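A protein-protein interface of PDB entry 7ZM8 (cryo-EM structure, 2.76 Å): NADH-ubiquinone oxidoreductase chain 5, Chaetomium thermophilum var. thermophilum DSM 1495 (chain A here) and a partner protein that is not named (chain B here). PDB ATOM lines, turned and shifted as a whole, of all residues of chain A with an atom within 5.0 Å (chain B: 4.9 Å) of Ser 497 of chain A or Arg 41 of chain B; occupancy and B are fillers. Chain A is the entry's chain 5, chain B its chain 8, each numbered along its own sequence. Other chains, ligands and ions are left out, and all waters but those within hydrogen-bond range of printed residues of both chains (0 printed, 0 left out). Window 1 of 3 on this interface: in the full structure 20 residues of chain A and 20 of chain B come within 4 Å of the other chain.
SG of Cys 51 of chain B forms a disulfide with SG of Cys 40 of chain B, 2.0 Å away. The backbone NH (N) of Tyr 46 of chain B sits at hydrogen-bond distance from the backbone carbonyl oxygen (O) of Arg 41 of chain B, 3.1 Å away. The guanidinium group (NH2) of Arg 41 of chain B sits at hydrogen-bond distance from the side-chain amide oxygen (OD1) of Asn 38 of chain B (3.0 Å). The backbone NH of Phe 499 of chain A is in hydrogen-bond range of the side-chain hydroxyl of Ser 497 of chain A (3.4 Å).
The side-chain carboxylate (OD2) of Asp 490 of chain A is in salt-bridge range of the guanidinium group (NE) of Arg 41 of chain B, 3.2 Å away. The side-chain amide nitrogen (ND2) of Asn 38 of chain B lies within hydrogen-bond range of the backbone carbonyl oxygen (O) of Gly 496 of chain A (2.8 Å). N of Ser 497 of chain A sits close to NH2 of Arg 41 of chain B, at 3.2 Å. The side-chain amide oxygen (OD1) of Asn 498 of chain A sits close to the side-chain hydroxyl (OH) of Tyr 46 of chain B, at 2.4 Å. OD2 of Asp 490 of chain A is in salt-bridge range of NH1 of Arg 55 of chain B.
Of the 15 printed residues of chain B, 6 touch a printed residue of chain A. Hydrophobic or aromatic side chains of chain B that line the printed part of chain A: Pro 23, Leu 34 and Tyr 46. Printed residues of chain A that touch a printed residue of chain B: Asp 490, Ile 491, Leu 495, Gly 496, Ser 497, Asn 498 and Phe 499.
Among the printed residues, pairs that only touch across the chains: Asp 490 of chain A with Tyr 46 of chain B, Ile 491 of chain A with Tyr 46 of chain B, Leu 495 of chain A with Arg 41 of chain B, Gly 496 of chain A with Leu 34 of chain B, Gly 496 of chain A with Arg 41 of chain B, Ser 497 of chain A with Pro 23 of chain B, Ser 497 of chain A with Asn 38 of chain B, Ser 497 of chain A with Tyr 46 of chain B, Asn 498 of chain A with Asn 38 of chain B and Phe 499 of chain A with Tyr 46 of chain B.
Of the printed residues of chain B, Leu 495 of chain A touches Arg 41. Of chain B, only Pro 23, Asn 38, Arg 41 and Tyr 46 come within 4 Å of Ser 497 of chain A. Printed residues of chain A within 4 Å of Leu 34 of chain B: Gly 496. The nearest printed residue of chain B that does not touch Ser 497 of chain A is Leu 34 of chain B (5.1 Å). The nearest printed residue of chain A that does not touch Asn 38 of chain B is Phe 499 of chain A (6.5 Å).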
ATOM      1  N   ASP A 490      24.301  24.937 -28.418  1.00  0.00           N
ATOM      2  CA  ASP A 490      23.407  25.553 -27.449  1.00  0.00           C
ATOM      3  C   ASP A 490      23.663  25.061 -26.033  1.00  0.00           C
ATOM      4  O   ASP A 490      23.585  25.847 -25.086  1.00  0.00           O
ATOM      5  CB  ASP A 490      21.961  25.284 -27.846  1.00  0.00           C
ATOM      6  CG  ASP A 490      21.013  26.295 -27.275  1.00  0.00           C
ATOM      7  OD1 ASP A 490      21.383  27.483 -27.231  1.00  0.00           O
ATOM      8  OD2 ASP A 490      19.902  25.904 -26.872  1.00  0.00           O
ATOM      9  N   ILE A 491      23.962  23.772 -25.872  1.00  0.00           N
ATOM     10  CA  ILE A 491      24.226  23.211 -24.552  1.00  0.00           C
ATOM     11  C   ILE A 491      25.424  23.885 -23.903  1.00  0.00           C
ATOM     12  O   ILE A 491      25.501  23.990 -22.674  1.00  0.00           O
ATOM     13  CB  ILE A 491      24.429  21.687 -24.675  1.00  0.00           C
ATOM     14  CG1 ILE A 491      23.159  21.025 -25.186  1.00  0.00           C
ATOM     15  CG2 ILE A 491      24.820  21.076 -23.349  1.00  0.00           C
ATOM     16  CD1 ILE A 491      23.350  19.592 -25.579  1.00  0.00           C
ATOM     17  N   ILE A 493      27.622  26.875 -25.674  1.00  0.00           N
ATOM     18  CA  ILE A 493      27.763  28.301 -25.945  1.00  0.00           C
ATOM     19  C   ILE A 493      26.527  29.030 -25.445  1.00  0.00           C
ATOM     20  O   ILE A 493      26.606  29.828 -24.504  1.00  0.00           O
ATOM     21  CB  ILE A 493      27.975  28.583 -27.442  1.00  0.00           C
ATOM     22  CG1 ILE A 493      29.149  27.779 -27.988  1.00  0.00           C
ATOM     23  CG2 ILE A 493      28.194  30.069 -27.673  1.00  0.00           C
ATOM     24  CD1 ILE A 493      30.455  28.124 -27.336  1.00  0.00           C
ATOM     25  N   GLY A 494      25.380  28.746 -26.057  1.00  0.00           N
ATOM     26  CA  GLY A 494      24.124  29.381 -25.709  1.00  0.00           C
ATOM     27  C   GLY A 494      24.192  30.892 -25.654  1.00  0.00           C
ATOM     28  O   GLY A 494      25.114  31.505 -26.199  1.00  0.00           O
ATOM     29  N   LEU A 495      23.221  31.502 -25.027  1.00  0.00           N
ATOM     30  CA  LEU A 495      23.374  32.897 -24.644  1.00  0.00           C
ATOM     31  C   LEU A 495      23.003  33.130 -23.190  1.00  0.00           C
ATOM     32  O   LEU A 495      23.647  33.934 -22.515  1.00  0.00           O
ATOM     33  CB  LEU A 495      22.542  33.801 -25.552  1.00  0.00           C
ATOM     34  CG  LEU A 495      22.827  35.288 -25.369  1.00  0.00           C
ATOM     35  CD1 LEU A 495      24.322  35.534 -25.382  1.00  0.00           C
ATOM     36  CD2 LEU A 495      22.142  36.105 -26.447  1.00  0.00           C
ATOM     37  N   GLY A 496      21.987  32.440 -22.693  1.00  0.00           N
ATOM     38  CA  GLY A 496      21.672  32.442 -21.284  1.00  0.00           C
ATOM     39  C   GLY A 496      21.393  31.025 -20.849  1.00  0.00           C
ATOM     40  O   GLY A 496      20.544  30.781 -19.992  1.00  0.00           O
ATOM     41  N   SER A 497      22.101  30.082 -21.464  1.00  0.00           N
ATOM     42  CA  SER A 497      21.807  28.671 -21.282  1.00  0.00           C
ATOM     43  C   SER A 497      21.960  28.268 -19.823  1.00  0.00           C
ATOM     44  O   SER A 497      22.842  28.752 -19.113  1.00  0.00           O
ATOM     45  CB  SER A 497      22.721  27.828 -22.168  1.00  0.00           C
ATOM     46  OG  SER A 497      22.806  26.495 -21.700  1.00  0.00           O
ATOM     47  N   ASN A 498      21.082  27.377 -19.379  1.00  0.00           N
ATOM     48  CA  ASN A 498      21.028  26.938 -17.994  1.00  0.00           C
ATOM     49  C   ASN A 498      21.463  25.484 -17.837  1.00  0.00           C
ATOM     50  O   ASN A 498      20.952  24.769 -16.975  1.00  0.00           O
ATOM     51  CB  ASN A 498      19.620  27.136 -17.441  1.00  0.00           C
ATOM     52  CG  ASN A 498      18.578  26.348 -18.208  1.00  0.00           C
ATOM     53  OD1 ASN A 498      18.787  25.976 -19.362  1.00  0.00           O
ATOM     54  ND2 ASN A 498      17.449  26.085 -17.565  1.00  0.00           N
ATOM     55  N   PHE A 499      22.403  25.026 -18.664  1.00  0.00           N
ATOM     56  CA  PHE A 499      22.829  23.636 -18.565  1.00  0.00           C
ATOM     57  C   PHE A 499      23.722  23.414 -17.355  1.00  0.00           C
ATOM     58  O   PHE A 499      23.691  22.339 -16.746  1.00  0.00           O
ATOM     59  CB  PHE A 499      23.544  23.197 -19.839  1.00  0.00           C
ATOM     60  CG  PHE A 499      23.541  21.712 -20.039  1.00  0.00           C
ATOM     61  CD1 PHE A 499      22.446  21.082 -20.593  1.00  0.00           C
ATOM     62  CD2 PHE A 499      24.619  20.944 -19.647  1.00  0.00           C
ATOM     63  CE1 PHE A 499      22.429  19.721 -20.763  1.00  0.00           C
ATOM     64  CE2 PHE A 499      24.609  19.583 -19.819  1.00  0.00           C
ATOM     65  CZ  PHE A 499      23.514  18.971 -20.376  1.00  0.00           C
ATOM     66  N   PRO B  23      20.843  31.889 -14.440  1.00  0.00           N
ATOM     67  CA  PRO B  23      22.250  32.111 -14.085  1.00  0.00           C
ATOM     68  C   PRO B  23      22.480  33.545 -13.632  1.00  0.00           C
ATOM     69  O   PRO B  23      21.875  34.481 -14.151  1.00  0.00           O
ATOM     70  CB  PRO B  23      22.993  31.798 -15.386  1.00  0.00           C
ATOM     71  CG  PRO B  23      22.086  30.857 -16.109  1.00  0.00           C
ATOM     72  CD  PRO B  23      20.701  31.328 -15.794  1.00  0.00           C
ATOM     73  N   LEU B  34      14.573  35.502 -20.951  1.00  0.00           N
ATOM     74  CA  LEU B  34      15.344  34.294 -20.709  1.00  0.00           C
ATOM     75  C   LEU B  34      14.530  33.227 -19.995  1.00  0.00           C
ATOM     76  O   LEU B  34      14.840  32.040 -20.130  1.00  0.00           O
ATOM     77  CB  LEU B  34      16.592  34.619 -19.896  1.00  0.00           C
ATOM     78  CG  LEU B  34      17.665  33.535 -19.870  1.00  0.00           C
ATOM     79  CD1 LEU B  34      17.971  33.080 -21.276  1.00  0.00           C
ATOM     80  CD2 LEU B  34      18.910  34.049 -19.187  1.00  0.00           C
ATOM     81  N   PRO B  36      11.281  32.148 -20.600  1.00  0.00           N
ATOM     82  CA  PRO B  36      10.726  31.195 -21.569  1.00  0.00           C
ATOM     83  C   PRO B  36      11.773  30.557 -22.462  1.00  0.00           C
ATOM     84  O   PRO B  36      11.586  29.410 -22.881  1.00  0.00           O
ATOM     85  CB  PRO B  36       9.747  32.052 -22.378  1.00  0.00           C
ATOM     86  CG  PRO B  36      10.295  33.408 -22.284  1.00  0.00           C
ATOM     87  CD  PRO B  36      10.835  33.519 -20.899  1.00  0.00           C
ATOM     88  N   LEU B  37      12.861  31.261 -22.773  1.00  0.00           N
ATOM     89  CA  LEU B  37      13.885  30.686 -23.639  1.00  0.00           C
ATOM     90  C   LEU B  37      14.504  29.449 -23.008  1.00  0.00           C
ATOM     91  O   LEU B  37      14.569  28.388 -23.634  1.00  0.00           O
ATOM     92  CB  LEU B  37      14.959  31.724 -23.951  1.00  0.00           C
ATOM     93  CG  LEU B  37      16.163  31.178 -24.719  1.00  0.00           C
ATOM     94  CD1 LEU B  37      15.724  30.535 -26.012  1.00  0.00           C
ATOM     95  CD2 LEU B  37      17.166  32.272 -24.984  1.00  0.00           C
ATOM     96  N   ASN B  38      14.967  29.565 -21.765  1.00  0.00           N
ATOM     97  CA  ASN B  38      15.498  28.400 -21.071  1.00  0.00           C
ATOM     98  C   ASN B  38      14.414  27.361 -20.828  1.00  0.00           C
ATOM     99  O   ASN B  38      14.715  26.172 -20.687  1.00  0.00           O
ATOM    100  CB  ASN B  38      16.143  28.827 -19.754  1.00  0.00           C
ATOM    101  CG  ASN B  38      17.520  29.416 -19.951  1.00  0.00           C
ATOM    102  OD1 ASN B  38      18.047  29.420 -21.058  1.00  0.00           O
ATOM    103  ND2 ASN B  38      18.108  29.929 -18.878  1.00  0.00           N
ATOM    104  N   ARG B  39      13.151  27.785 -20.771  1.00  0.00           N
ATOM    105  CA  ARG B  39      12.049  26.834 -20.689  1.00  0.00           C
ATOM    106  C   ARG B  39      11.852  26.105 -22.009  1.00  0.00           C
ATOM    107  O   ARG B  39      11.603  24.896 -22.024  1.00  0.00           O
ATOM    108  CB  ARG B  39      10.768  27.555 -20.281  1.00  0.00           C
ATOM    109  CG  ARG B  39       9.548  26.661 -20.203  1.00  0.00           C
ATOM    110  CD  ARG B  39       9.487  25.938 -18.871  1.00  0.00           C
ATOM    111  NE  ARG B  39       8.805  24.654 -18.975  1.00  0.00           N
ATOM    112  CZ  ARG B  39       9.154  23.568 -18.296  1.00  0.00           C
ATOM    113  NH1 ARG B  39      10.187  23.607 -17.465  1.00  0.00           N
ATOM    114  NH2 ARG B  39       8.475  22.440 -18.450  1.00  0.00           N
ATOM    115  N   CYS B  40      11.942  26.828 -23.127  1.00  0.00           N
ATOM    116  CA  CYS B  40      11.851  26.195 -24.438  1.00  0.00           C
ATOM    117  C   CYS B  40      13.027  25.263 -24.678  1.00  0.00           C
ATOM    118  O   CYS B  40      12.861  24.188 -25.262  1.00  0.00           O
ATOM    119  CB  CYS B  40      11.785  27.258 -25.528  1.00  0.00           C
ATOM    120  SG  CYS B  40      11.315  26.654 -27.172  1.00  0.00           S
ATOM    121  N   ARG B  41      14.223  25.662 -24.249  1.00  0.00           N
ATOM    122  CA  ARG B  41      15.387  24.794 -24.367  1.00  0.00           C
ATOM    123  C   ARG B  41      15.209  23.507 -23.580  1.00  0.00           C
ATOM    124  O   ARG B  41      15.676  22.448 -24.011  1.00  0.00           O
ATOM    125  CB  ARG B  41      16.634  25.537 -23.898  1.00  0.00           C
ATOM    126  CG  ARG B  41      17.106  26.602 -24.855  1.00  0.00           C
ATOM    127  CD  ARG B  41      18.137  27.478 -24.207  1.00  0.00           C
ATOM    128  NE  ARG B  41      18.757  28.388 -25.155  1.00  0.00           N
ATOM    129  CZ  ARG B  41      19.493  29.433 -24.805  1.00  0.00           C
ATOM    130  NH1 ARG B  41      20.037  30.207 -25.728  1.00  0.00           N
ATOM    131  NH2 ARG B  41      19.651  29.723 -23.527  1.00  0.00           N
ATOM    132  N   TYR B  42      14.549  23.575 -22.426  1.00  0.00           N
ATOM    133  CA  TYR B  42      14.321  22.369 -21.639  1.00  0.00           C
ATOM    134  C   TYR B  42      13.404  21.404 -22.376  1.00  0.00           C
ATOM    135  O   TYR B  42      13.691  20.205 -22.470  1.00  0.00           O
ATOM    136  CB  TYR B  42      13.734  22.739 -20.277  1.00  0.00           C
ATOM    137  CG  TYR B  42      12.956  21.622 -19.623  1.00  0.00           C
ATOM    138  CD1 TYR B  42      13.593  20.669 -18.847  1.00  0.00           C
ATOM    139  CD2 TYR B  42      11.587  21.522 -19.785  1.00  0.00           C
ATOM    140  CE1 TYR B  42      12.888  19.651 -18.253  1.00  0.00           C
ATOM    141  CE2 TYR B  42      10.877  20.505 -19.205  1.00  0.00           C
ATOM    142  CZ  TYR B  42      11.529  19.575 -18.438  1.00  0.00           C
ATOM    143  OH  TYR B  42      10.808  18.563 -17.860  1.00  0.00           O
ATOM    144  N   GLU B  43      12.293  21.910 -22.910  1.00  0.00           N
ATOM    145  CA  GLU B  43      11.336  21.041 -23.575  1.00  0.00           C
ATOM    146  C   GLU B  43      11.852  20.512 -24.900  1.00  0.00           C
ATOM    147  O   GLU B  43      11.395  19.459 -25.350  1.00  0.00           O
ATOM    148  CB  GLU B  43      10.018  21.782 -23.795  1.00  0.00           C
ATOM    149  CG  GLU B  43       9.274  22.116 -22.514  1.00  0.00           C
ATOM    150  CD  GLU B  43       7.983  22.866 -22.770  1.00  0.00           C
ATOM    151  OE1 GLU B  43       7.731  23.234 -23.937  1.00  0.00           O
ATOM    152  OE2 GLU B  43       7.220  23.088 -21.807  1.00  0.00           O
ATOM    153  N   THR B  44      12.787  21.212 -25.533  1.00  0.00           N
ATOM    154  CA  THR B  44      13.236  20.872 -26.873  1.00  0.00           C
ATOM    155  C   THR B  44      14.623  20.250 -26.891  1.00  0.00           C
ATOM    156  O   THR B  44      15.163  20.011 -27.971  1.00  0.00           O
ATOM    157  CB  THR B  44      13.210  22.114 -27.754  1.00  0.00           C
ATOM    158  OG1 THR B  44      13.978  23.148 -27.134  1.00  0.00           O
ATOM    159  CG2 THR B  44      11.786  22.598 -27.884  1.00  0.00           C
ATOM    160  N   TYR B  45      15.203  19.980 -25.720  1.00  0.00           N
ATOM    161  CA  TYR B  45      16.511  19.335 -25.588  1.00  0.00           C
ATOM    162  C   TYR B  45      17.624  20.129 -26.263  1.00  0.00           C
ATOM    163  O   TYR B  45      18.579  19.551 -26.780  1.00  0.00           O
ATOM    164  CB  TYR B  45      16.479  17.901 -26.119  1.00  0.00           C
ATOM    165  CG  TYR B  45      15.842  16.927 -25.166  1.00  0.00           C
ATOM    166  CD1 TYR B  45      14.465  16.759 -25.128  1.00  0.00           C
ATOM    167  CD2 TYR B  45      16.614  16.188 -24.290  1.00  0.00           C
ATOM    168  CE1 TYR B  45      13.885  15.877 -24.252  1.00  0.00           C
ATOM    169  CE2 TYR B  45      16.041  15.308 -23.413  1.00  0.00           C
ATOM    170  CZ  TYR B  45      14.679  15.154 -23.394  1.00  0.00           C
ATOM    171  OH  TYR B  45      14.117  14.266 -22.512  1.00  0.00           O
ATOM    172  N   TYR B  46      17.511  21.457 -26.250  1.00  0.00           N
ATOM    173  CA  TYR B  46      18.552  22.365 -26.740  1.00  0.00           C
ATOM    174  C   TYR B  46      18.891  22.129 -28.205  1.00  0.00           C
ATOM    175  O   TYR B  46      20.018  22.378 -28.636  1.00  0.00           O
ATOM    176  CB  TYR B  46      19.829  22.269 -25.898  1.00  0.00           C
ATOM    177  CG  TYR B  46      19.681  22.718 -24.474  1.00  0.00           C
ATOM    178  CD1 TYR B  46      19.148  21.875 -23.514  1.00  0.00           C
ATOM    179  CD2 TYR B  46      20.071  23.987 -24.088  1.00  0.00           C
ATOM    180  CE1 TYR B  46      19.011  22.283 -22.210  1.00  0.00           C
ATOM    181  CE2 TYR B  46      19.941  24.406 -22.784  1.00  0.00           C
ATOM    182  CZ  TYR B  46      19.412  23.548 -21.848  1.00  0.00           C
ATOM    183  OH  TYR B  46      19.276  23.961 -20.547  1.00  0.00           O
ATOM    184  N   CYS B  51      13.768  26.355 -31.071  1.00  0.00           N
ATOM    185  CA  CYS B  51      13.303  27.486 -30.276  1.00  0.00           C
ATOM    186  C   CYS B  51      13.776  28.803 -30.876  1.00  0.00           C
ATOM    187  O   CYS B  51      14.190  29.716 -30.163  1.00  0.00           O
ATOM    188  CB  CYS B  51      13.767  27.355 -28.828  1.00  0.00           C
ATOM    189  SG  CYS B  51      13.049  25.949 -27.964  1.00  0.00           S
ATOM    190  N   ARG B  55      14.873  32.574 -28.939  1.00  0.00           N
ATOM    191  CA  ARG B  55      16.245  33.067 -28.952  1.00  0.00           C
ATOM    192  C   ARG B  55      16.313  34.445 -29.582  1.00  0.00           C
ATOM    193  O   ARG B  55      16.990  35.339 -29.065  1.00  0.00           O
ATOM    194  CB  ARG B  55      17.161  32.107 -29.703  1.00  0.00           C
ATOM    195  CG  ARG B  55      17.040  30.674 -29.292  1.00  0.00           C
ATOM    196  CD  ARG B  55      17.785  29.765 -30.242  1.00  0.00           C
ATOM    197  NE  ARG B  55      17.608  28.367 -29.875  1.00  0.00           N
ATOM    198  CZ  ARG B  55      18.201  27.797 -28.834  1.00  0.00           C
ATOM    199  NH1 ARG B  55      17.985  26.519 -28.563  1.00  0.00           N
ATOM    200  NH2 ARG B  55      19.008  28.507 -28.067  1.00  0.00           N
